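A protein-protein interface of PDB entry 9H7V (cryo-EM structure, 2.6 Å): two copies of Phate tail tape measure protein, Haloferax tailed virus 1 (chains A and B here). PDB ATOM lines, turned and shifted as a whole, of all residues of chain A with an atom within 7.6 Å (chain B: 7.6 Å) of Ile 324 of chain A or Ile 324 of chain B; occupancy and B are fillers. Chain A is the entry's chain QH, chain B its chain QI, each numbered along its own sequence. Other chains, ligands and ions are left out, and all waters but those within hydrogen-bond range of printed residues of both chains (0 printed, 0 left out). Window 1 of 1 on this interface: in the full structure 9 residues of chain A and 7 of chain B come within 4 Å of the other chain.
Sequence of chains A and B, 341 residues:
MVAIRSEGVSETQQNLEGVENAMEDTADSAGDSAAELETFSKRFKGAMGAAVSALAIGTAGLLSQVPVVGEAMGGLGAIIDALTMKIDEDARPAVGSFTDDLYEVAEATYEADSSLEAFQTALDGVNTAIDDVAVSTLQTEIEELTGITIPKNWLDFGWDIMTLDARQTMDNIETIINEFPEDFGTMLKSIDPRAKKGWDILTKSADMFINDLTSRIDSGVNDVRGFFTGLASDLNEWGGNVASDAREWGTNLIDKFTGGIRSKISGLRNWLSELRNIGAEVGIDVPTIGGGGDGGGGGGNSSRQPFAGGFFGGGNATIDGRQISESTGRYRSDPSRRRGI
O of Thr 318 of chain A lies within hydrogen-bond range of N of Glu 326 of chain B, 3.0 Å away. The side-chain carboxylate (OE2) of Glu 326 of chain A is in salt-bridge range of the guanidinium group (NH1) of Arg 322 of chain B. O of Ile 324 of chain B lies within hydrogen-bond range of N of Asp 320 of chain A, at 2.8 Å. The side-chain amide nitrogen (NE2) of Gln 323 of chain A is in hydrogen-bond range of the backbone carbonyl oxygen (O) of Gln 323 of chain B, at 3.0 Å. The side-chain carboxylate (OD2) of Asp 320 of chain B lies within hydrogen-bond range of the side-chain hydroxyl (OH) of Tyr 331 of chain A. The side-chain hydroxyl of Ser 327 of chain A is in hydrogen-bond range of the guanidinium group of Arg 322 of chain B (3.4 Å).
Thr 318 of chain A touches Ser 325 of chain B, but with the chains exchanged Ser 325 of chain A does not touch Thr 318 of chain B (11.0 Å). Thr 318 of chain A touches Glu 326 of chain B, but with the chains exchanged Glu 326 of chain A does not touch Thr 318 of chain B (11.0 Å). Ile 319 of chain A touches Ile 324 of chain B, but with the chains exchanged Ile 324 of chain A does not touch Ile 319 of chain B (4.4 Å). Asp 320 of chain A touches Glu 326 of chain B, but with the chains exchanged Glu 326 of chain A does not touch Asp 320 of chain B (8.4 Å). Of the 11 pairs that touch across the chains among the printed residues, 2 have their exchanged pair printed and touching as well.
Ser 325 of chain B touches Thr 318 of chain A (CA to O, 3.5 Å). CA of Ile 319 of chain A touches O of Ile 324 of chain B (3.5 Å). OD2 of Asp 320 of chain A touches CG of Glu 326 of chain B, at 3.97 Å. CG1 of Ile 324 of chain A touches CG2 of Ile 324 of chain B (3.9 Å). CG2 of Ile 319 of chain B touches CB of Ser 327 of chain A, 3.97 Å away.
Hydrophobic or aromatic side chains of chain B within 4 Å of the printed part of chain A: Ile 319 and Ile 324.
OD1 of Asp 320 of chain A lies within hydrogen-bond range of N of Arg 322 of chain A, at 2.9 Å. OE1 of Gln 323 of chain B lies within hydrogen-bond range of ND2 of Asn 316 of chain B (2.9 Å). The backbone carbonyl oxygen (O) of Ala 317 of chain B is in hydrogen-bond range of the backbone NH (N) of Ile 324 of chain B, at 3.0 Å. The side-chain carboxylate (OD1) of Asp 320 of chain A lies within hydrogen-bond range of the backbone NH (N) of Gln 323 of chain A (3.2 Å). The side-chain hydroxyl of Thr 328 of chain A sits at hydrogen-bond distance from the backbone carbonyl oxygen of Ile 324 of chain A (2.8 Å). N of Ala 317 of chain B sits at hydrogen-bond distance from OG of Ser 325 of chain B (3.4 Å).
Ile 324 of chain A touches just one residue of chain B: Ile 324 (3.9 Å). Of the printed residues of chain B, Ile 319 of chain A touches Ile 324 (3.5 Å). Of the printed residues of chain B, Ser 327 of chain A touches Ile 319 (3.97 Å) and Arg 322 (3.4 Å). Printed residues of chain B within 4 Å of Asp 320 of chain A: Ile 324 and Glu 326. Printed residues of chain B within 4 Å of Thr 318 of chain A: Ser 325 (3.5 Å) and Glu 326 (3.0 Å). Arg 322 of chain A touches none of the printed residues of chain B. Ala 317 of chain A touches none of the printed residues of chain B. The nearest residue of chain A that does not touch Ile 324 of chain B is Gln 323 of chain A (4.03 Å).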
ATOM      1  N   ALA A 317      20.041 -38.567  11.721  1.00  0.00           N
ATOM      2  CA  ALA A 317      20.647 -37.296  12.212  1.00  0.00           C
ATOM      3  C   ALA A 317      22.121 -37.526  12.544  1.00  0.00           C
ATOM      4  O   ALA A 317      22.443 -38.143  13.559  1.00  0.00           O
ATOM      5  CB  ALA A 317      19.870 -36.779  13.401  1.00  0.00           C
ATOM      6  N   THR A 318      23.001 -37.028  11.666  1.00  0.00           N
ATOM      7  CA  THR A 318      24.441 -37.185  11.816  1.00  0.00           C
ATOM      8  C   THR A 318      25.029 -35.915  12.429  1.00  0.00           C
ATOM      9  O   THR A 318      24.904 -34.831  11.860  1.00  0.00           O
ATOM     10  CB  THR A 318      25.108 -37.581  10.490  1.00  0.00           C
ATOM     11  OG1 THR A 318      24.404 -38.695   9.941  1.00  0.00           O
ATOM     12  CG2 THR A 318      26.571 -37.939  10.642  1.00  0.00           C
ATOM     13  N   ILE A 319      25.682 -36.084  13.585  1.00  0.00           N
ATOM     14  CA  ILE A 319      26.200 -34.986  14.386  1.00  0.00           C
ATOM     15  C   ILE A 319      27.720 -34.924  14.225  1.00  0.00           C
ATOM     16  O   ILE A 319      28.402 -35.944  14.325  1.00  0.00           O
ATOM     17  CB  ILE A 319      25.763 -35.133  15.862  1.00  0.00           C
ATOM     18  CG1 ILE A 319      24.239 -35.199  16.038  1.00  0.00           C
ATOM     19  CG2 ILE A 319      26.397 -34.071  16.749  1.00  0.00           C
ATOM     20  CD1 ILE A 319      23.475 -33.944  15.643  1.00  0.00           C
ATOM     21  N   ASP A 320      28.226 -33.707  13.980  1.00  0.00           N
ATOM     22  CA  ASP A 320      29.640 -33.438  13.774  1.00  0.00           C
ATOM     23  C   ASP A 320      30.309 -33.199  15.126  1.00  0.00           C
ATOM     24  O   ASP A 320      29.957 -32.261  15.842  1.00  0.00           O
ATOM     25  CB  ASP A 320      29.836 -32.265  12.806  1.00  0.00           C
ATOM     26  CG  ASP A 320      31.273 -32.013  12.374  1.00  0.00           C
ATOM     27  OD1 ASP A 320      32.182 -32.102  13.225  1.00  0.00           O
ATOM     28  OD2 ASP A 320      31.474 -31.713  11.181  1.00  0.00           O
ATOM     29  N   GLY A 321      31.287 -34.057  15.440  1.00  0.00           N
ATOM     30  CA  GLY A 321      31.998 -34.047  16.710  1.00  0.00           C
ATOM     31  C   GLY A 321      32.923 -32.843  16.871  1.00  0.00           C
ATOM     32  O   GLY A 321      33.104 -32.362  17.988  1.00  0.00           O
ATOM     33  N   ARG A 322      33.517 -32.380  15.761  1.00  0.00           N
ATOM     34  CA  ARG A 322      34.379 -31.207  15.778  1.00  0.00           C
ATOM     35  C   ARG A 322      33.550 -29.962  16.074  1.00  0.00           C
ATOM     36  O   ARG A 322      33.982 -29.110  16.843  1.00  0.00           O
ATOM     37  CB  ARG A 322      35.164 -31.061  14.471  1.00  0.00           C
ATOM     38  CG  ARG A 322      36.369 -31.985  14.379  1.00  0.00           C
ATOM     39  CD  ARG A 322      37.241 -31.821  13.153  1.00  0.00           C
ATOM     40  NE  ARG A 322      38.053 -33.016  12.955  1.00  0.00           N
ATOM     41  CZ  ARG A 322      39.328 -33.162  13.313  1.00  0.00           C
ATOM     42  NH1 ARG A 322      39.946 -34.307  13.077  1.00  0.00           N
ATOM     43  NH2 ARG A 322      39.986 -32.171  13.887  1.00  0.00           N
ATOM     44  N   GLN A 323      32.356 -29.894  15.469  1.00  0.00           N
ATOM     45  CA  GLN A 323      31.449 -28.770  15.628  1.00  0.00           C
ATOM     46  C   GLN A 323      30.972 -28.673  17.076  1.00  0.00           C
ATOM     47  O   GLN A 323      30.982 -27.581  17.637  1.00  0.00           O
ATOM     48  CB  GLN A 323      30.292 -28.841  14.627  1.00  0.00           C
ATOM     49  CG  GLN A 323      30.700 -28.570  13.183  1.00  0.00           C
ATOM     50  CD  GLN A 323      31.191 -27.163  12.937  1.00  0.00           C
ATOM     51  OE1 GLN A 323      32.378 -26.929  12.723  1.00  0.00           O
ATOM     52  NE2 GLN A 323      30.274 -26.208  12.968  1.00  0.00           N
ATOM     53  N   ILE A 324      30.577 -29.809  17.675  1.00  0.00           N
ATOM     54  CA  ILE A 324      30.095 -29.834  19.050  1.00  0.00           C
ATOM     55  C   ILE A 324      31.214 -29.409  20.002  1.00  0.00           C
ATOM     56  O   ILE A 324      31.007 -28.525  20.832  1.00  0.00           O
ATOM     57  CB  ILE A 324      29.446 -31.186  19.433  1.00  0.00           C
ATOM     58  CG1 ILE A 324      28.002 -31.264  18.926  1.00  0.00           C
ATOM     59  CG2 ILE A 324      29.535 -31.453  20.935  1.00  0.00           C
ATOM     60  CD1 ILE A 324      27.121 -32.268  19.643  1.00  0.00           C
ATOM     61  N   SER A 325      32.394 -30.025  19.852  1.00  0.00           N
ATOM     62  CA  SER A 325      33.503 -29.825  20.774  1.00  0.00           C
ATOM     63  C   SER A 325      34.055 -28.402  20.683  1.00  0.00           C
ATOM     64  O   SER A 325      34.478 -27.843  21.692  1.00  0.00           O
ATOM     65  CB  SER A 325      34.581 -30.852  20.566  1.00  0.00           C
ATOM     66  OG  SER A 325      35.079 -30.782  19.241  1.00  0.00           O
ATOM     67  N   GLU A 326      34.028 -27.824  19.474  1.00  0.00           N
ATOM     68  CA  GLU A 326      34.534 -26.484  19.223  1.00  0.00           C
ATOM     69  C   GLU A 326      33.534 -25.435  19.712  1.00  0.00           C
ATOM     70  O   GLU A 326      33.939 -24.370  20.176  1.00  0.00           O
ATOM     71  CB  GLU A 326      34.852 -26.331  17.736  1.00  0.00           C
ATOM     72  CG  GLU A 326      35.658 -25.099  17.381  1.00  0.00           C
ATOM     73  CD  GLU A 326      35.886 -24.981  15.886  1.00  0.00           C
ATOM     74  OE1 GLU A 326      36.782 -25.678  15.368  1.00  0.00           O
ATOM     75  OE2 GLU A 326      35.152 -24.209  15.237  1.00  0.00           O
ATOM     76  N   SER A 327      32.234 -25.745  19.603  1.00  0.00           N
ATOM     77  CA  SER A 327      31.172 -24.839  20.016  1.00  0.00           C
ATOM     78  C   SER A 327      31.050 -24.782  21.539  1.00  0.00           C
ATOM     79  O   SER A 327      30.713 -23.732  22.083  1.00  0.00           O
ATOM     80  CB  SER A 327      29.854 -25.193  19.376  1.00  0.00           C
ATOM     81  OG  SER A 327      29.928 -25.069  17.963  1.00  0.00           O
ATOM     82  N   THR A 328      31.326 -25.907  22.213  1.00  0.00           N
ATOM     83  CA  THR A 328      31.087 -26.025  23.646  1.00  0.00           C
ATOM     84  C   THR A 328      32.297 -25.572  24.467  1.00  0.00           C
ATOM     85  O   THR A 328      32.182 -25.437  25.684  1.00  0.00           O
ATOM     86  CB  THR A 328      30.612 -27.429  24.051  1.00  0.00           C
ATOM     87  OG1 THR A 328      31.523 -28.407  23.547  1.00  0.00           O
ATOM     88  CG2 THR A 328      29.204 -27.740  23.592  1.00  0.00           C
ATOM     89  N   GLY A 329      33.436 -25.326  23.803  1.00  0.00           N
ATOM     90  CA  GLY A 329      34.703 -25.009  24.453  1.00  0.00           C
ATOM     91  C   GLY A 329      34.623 -23.807  25.394  1.00  0.00           C
ATOM     92  O   GLY A 329      35.240 -23.813  26.458  1.00  0.00           O
ATOM     93  N   TYR A 331      32.127 -22.863  27.126  1.00  0.00           N
ATOM     94  CA  TYR A 331      31.373 -23.215  28.314  1.00  0.00           C
ATOM     95  C   TYR A 331      32.157 -24.205  29.173  1.00  0.00           C
ATOM     96  O   TYR A 331      31.985 -24.219  30.388  1.00  0.00           O
ATOM     97  CB  TYR A 331      29.977 -23.702  27.915  1.00  0.00           C
ATOM     98  CG  TYR A 331      29.214 -22.772  27.002  1.00  0.00           C
ATOM     99  CD1 TYR A 331      28.844 -21.501  27.420  1.00  0.00           C
ATOM    100  CD2 TYR A 331      28.863 -23.155  25.716  1.00  0.00           C
ATOM    101  CE1 TYR A 331      28.136 -20.642  26.593  1.00  0.00           C
ATOM    102  CE2 TYR A 331      28.155 -22.309  24.874  1.00  0.00           C
ATOM    103  CZ  TYR A 331      27.788 -21.048  25.316  1.00  0.00           C
ATOM    104  OH  TYR A 331      27.097 -20.201  24.500  1.00  0.00           O
ATOM    105  N   ARG A 332      33.013 -25.022  28.538  1.00  0.00           N
ATOM    106  CA  ARG A 332      33.820 -26.017  29.233  1.00  0.00           C
ATOM    107  C   ARG A 332      34.899 -25.343  30.080  1.00  0.00           C
ATOM    108  O   ARG A 332      35.243 -25.846  31.148  1.00  0.00           O
ATOM    109  CB  ARG A 332      34.460 -27.007  28.254  1.00  0.00           C
ATOM    110  CG  ARG A 332      33.492 -27.982  27.597  1.00  0.00           C
ATOM    111  CD  ARG A 332      34.174 -29.229  27.060  1.00  0.00           C
ATOM    112  NE  ARG A 332      35.412 -28.969  26.331  1.00  0.00           N
ATOM    113  CZ  ARG A 332      35.504 -28.720  25.027  1.00  0.00           C
ATOM    114  NH1 ARG A 332      36.687 -28.497  24.483  1.00  0.00           N
ATOM    115  NH2 ARG A 332      34.420 -28.698  24.271  1.00  0.00           N
ATOM    116  N   ASN B 316      18.502 -30.922  11.399  1.00  0.00           N
ATOM    117  CA  ASN B 316      19.202 -29.604  11.413  1.00  0.00           C
ATOM    118  C   ASN B 316      19.154 -29.031  12.828  1.00  0.00           C
ATOM    119  O   ASN B 316      18.081 -28.689  13.322  1.00  0.00           O
ATOM    120  CB  ASN B 316      18.615 -28.644  10.371  1.00  0.00           C
ATOM    121  CG  ASN B 316      19.485 -27.433  10.103  1.00  0.00           C
ATOM    122  OD1 ASN B 316      19.847 -26.695  11.018  1.00  0.00           O
ATOM    123  ND2 ASN B 316      19.816 -27.210   8.842  1.00  0.00           N
ATOM    124  N   ALA B 317      20.332 -28.926  13.461  1.00  0.00           N
ATOM    125  CA  ALA B 317      20.458 -28.515  14.854  1.00  0.00           C
ATOM    126  C   ALA B 317      21.619 -27.534  15.022  1.00  0.00           C
ATOM    127  O   ALA B 317      22.642 -27.671  14.354  1.00  0.00           O
ATOM    128  CB  ALA B 317      20.632 -29.730  15.731  1.00  0.00           C
ATOM    129  N   THR B 318      21.449 -26.556  15.929  1.00  0.00           N
ATOM    130  CA  THR B 318      22.412 -25.474  16.105  1.00  0.00           C
ATOM    131  C   THR B 318      22.772 -25.259  17.577  1.00  0.00           C
ATOM    132  O   THR B 318      21.923 -25.396  18.457  1.00  0.00           O
ATOM    133  CB  THR B 318      21.926 -24.157  15.478  1.00  0.00           C
ATOM    134  OG1 THR B 318      20.709 -23.748  16.104  1.00  0.00           O
ATOM    135  CG2 THR B 318      21.737 -24.222  13.977  1.00  0.00           C
ATOM    136  N   ILE B 319      24.052 -24.924  17.816  1.00  0.00           N
ATOM    137  CA  ILE B 319      24.544 -24.331  19.054  1.00  0.00           C
ATOM    138  C   ILE B 319      25.074 -22.940  18.710  1.00  0.00           C
ATOM    139  O   ILE B 319      25.985 -22.821  17.890  1.00  0.00           O
ATOM    140  CB  ILE B 319      25.641 -25.199  19.717  1.00  0.00           C
ATOM    141  CG1 ILE B 319      25.132 -26.592  20.107  1.00  0.00           C
ATOM    142  CG2 ILE B 319      26.267 -24.474  20.905  1.00  0.00           C
ATOM    143  CD1 ILE B 319      26.216 -27.570  20.518  1.00  0.00           C
ATOM    144  N   ASP B 320      24.493 -21.903  19.337  1.00  0.00           N
ATOM    145  CA  ASP B 320      24.874 -20.508  19.148  1.00  0.00           C
ATOM    146  C   ASP B 320      24.796 -20.109  17.672  1.00  0.00           C
ATOM    147  O   ASP B 320      25.564 -19.259  17.216  1.00  0.00           O
ATOM    148  CB  ASP B 320      26.238 -20.193  19.777  1.00  0.00           C
ATOM    149  CG  ASP B 320      26.175 -19.920  21.269  1.00  0.00           C
ATOM    150  OD1 ASP B 320      25.798 -18.792  21.644  1.00  0.00           O
ATOM    151  OD2 ASP B 320      26.495 -20.842  22.042  1.00  0.00           O
ATOM    152  N   GLY B 321      23.873 -20.734  16.930  1.00  0.00           N
ATOM    153  CA  GLY B 321      23.620 -20.374  15.543  1.00  0.00           C
ATOM    154  C   GLY B 321      24.521 -21.089  14.535  1.00  0.00           C
ATOM    155  O   GLY B 321      24.292 -20.969  13.332  1.00  0.00           O
ATOM    156  N   ARG B 322      25.547 -21.809  15.014  1.00  0.00           N
ATOM    157  CA  ARG B 322      26.351 -22.661  14.149  1.00  0.00           C
ATOM    158  C   ARG B 322      25.722 -24.049  14.093  1.00  0.00           C
ATOM    159  O   ARG B 322      25.250 -24.550  15.110  1.00  0.00           O
ATOM    160  CB  ARG B 322      27.787 -22.804  14.666  1.00  0.00           C
ATOM    161  CG  ARG B 322      28.678 -21.599  14.403  1.00  0.00           C
ATOM    162  CD  ARG B 322      30.109 -21.986  14.072  1.00  0.00           C
ATOM    163  NE  ARG B 322      30.765 -22.730  15.142  1.00  0.00           N
ATOM    164  CZ  ARG B 322      32.019 -23.176  15.120  1.00  0.00           C
ATOM    165  NH1 ARG B 322      32.494 -23.842  16.159  1.00  0.00           N
ATOM    166  NH2 ARG B 322      32.796 -22.958  14.072  1.00  0.00           N
ATOM    167  N   GLN B 323      25.763 -24.674  12.909  1.00  0.00           N
ATOM    168  CA  GLN B 323      25.201 -26.004  12.723  1.00  0.00           C
ATOM    169  C   GLN B 323      26.151 -27.067  13.269  1.00  0.00           C
ATOM    170  O   GLN B 323      27.360 -27.005  13.046  1.00  0.00           O
ATOM    171  CB  GLN B 323      24.832 -26.250  11.259  1.00  0.00           C
ATOM    172  CG  GLN B 323      23.514 -25.595  10.867  1.00  0.00           C
ATOM    173  CD  GLN B 323      23.061 -25.837   9.447  1.00  0.00           C
ATOM    174  OE1 GLN B 323      22.035 -25.316   9.014  1.00  0.00           O
ATOM    175  NE2 GLN B 323      23.818 -26.626   8.701  1.00  0.00           N
ATOM    176  N   ILE B 324      25.565 -28.038  13.982  1.00  0.00           N
ATOM    177  CA  ILE B 324      26.281 -29.185  14.523  1.00  0.00           C
ATOM    178  C   ILE B 324      25.971 -30.439  13.703  1.00  0.00           C
ATOM    179  O   ILE B 324      26.499 -31.512  13.999  1.00  0.00           O
ATOM    180  CB  ILE B 324      26.028 -29.371  16.038  1.00  0.00           C
ATOM    181  CG1 ILE B 324      24.538 -29.473  16.389  1.00  0.00           C
ATOM    182  CG2 ILE B 324      26.735 -28.283  16.837  1.00  0.00           C
ATOM    183  CD1 ILE B 324      24.243 -30.236  17.664  1.00  0.00           C
ATOM    184  N   SER B 325      25.123 -30.298  12.673  1.00  0.00           N
ATOM    185  CA  SER B 325      24.872 -31.356  11.706  1.00  0.00           C
ATOM    186  C   SER B 325      26.076 -31.482  10.774  1.00  0.00           C
ATOM    187  O   SER B 325      26.626 -30.471  10.338  1.00  0.00           O
ATOM    188  CB  SER B 325      23.611 -31.087  10.923  1.00  0.00           C
ATOM    189  OG  SER B 325      22.485 -31.005  11.783  1.00  0.00           O
ATOM    190  N   GLU B 326      26.475 -32.724  10.477  1.00  0.00           N
ATOM    191  CA  GLU B 326      27.605 -32.969   9.595  1.00  0.00           C
ATOM    192  C   GLU B 326      27.164 -32.810   8.142  1.00  0.00           C
ATOM    193  O   GLU B 326      26.074 -33.241   7.771  1.00  0.00           O
ATOM    194  CB  GLU B 326      28.206 -34.353   9.850  1.00  0.00           C
ATOM    195  CG  GLU B 326      29.559 -34.557   9.187  1.00  0.00           C
ATOM    196  CD  GLU B 326      30.324 -35.813   9.572  1.00  0.00           C
ATOM    197  OE1 GLU B 326      29.759 -36.665  10.290  1.00  0.00           O
ATOM    198  OE2 GLU B 326      31.488 -35.940   9.147  1.00  0.00           O
ATOM    199  N   SER B 327      28.033 -32.189   7.334  1.00  0.00           N
ATOM    200  CA  SER B 327      27.828 -32.096   5.898  1.00  0.00           C
ATOM    201  C   SER B 327      28.332 -33.370   5.222  1.00  0.00           C
ATOM    202  O   SER B 327      29.237 -33.327   4.388  1.00  0.00           O
ATOM    203  CB  SER B 327      28.457 -30.849   5.326  1.00  0.00           C
ATOM    204  OG  SER B 327      28.012 -30.627   3.996  1.00  0.00           O
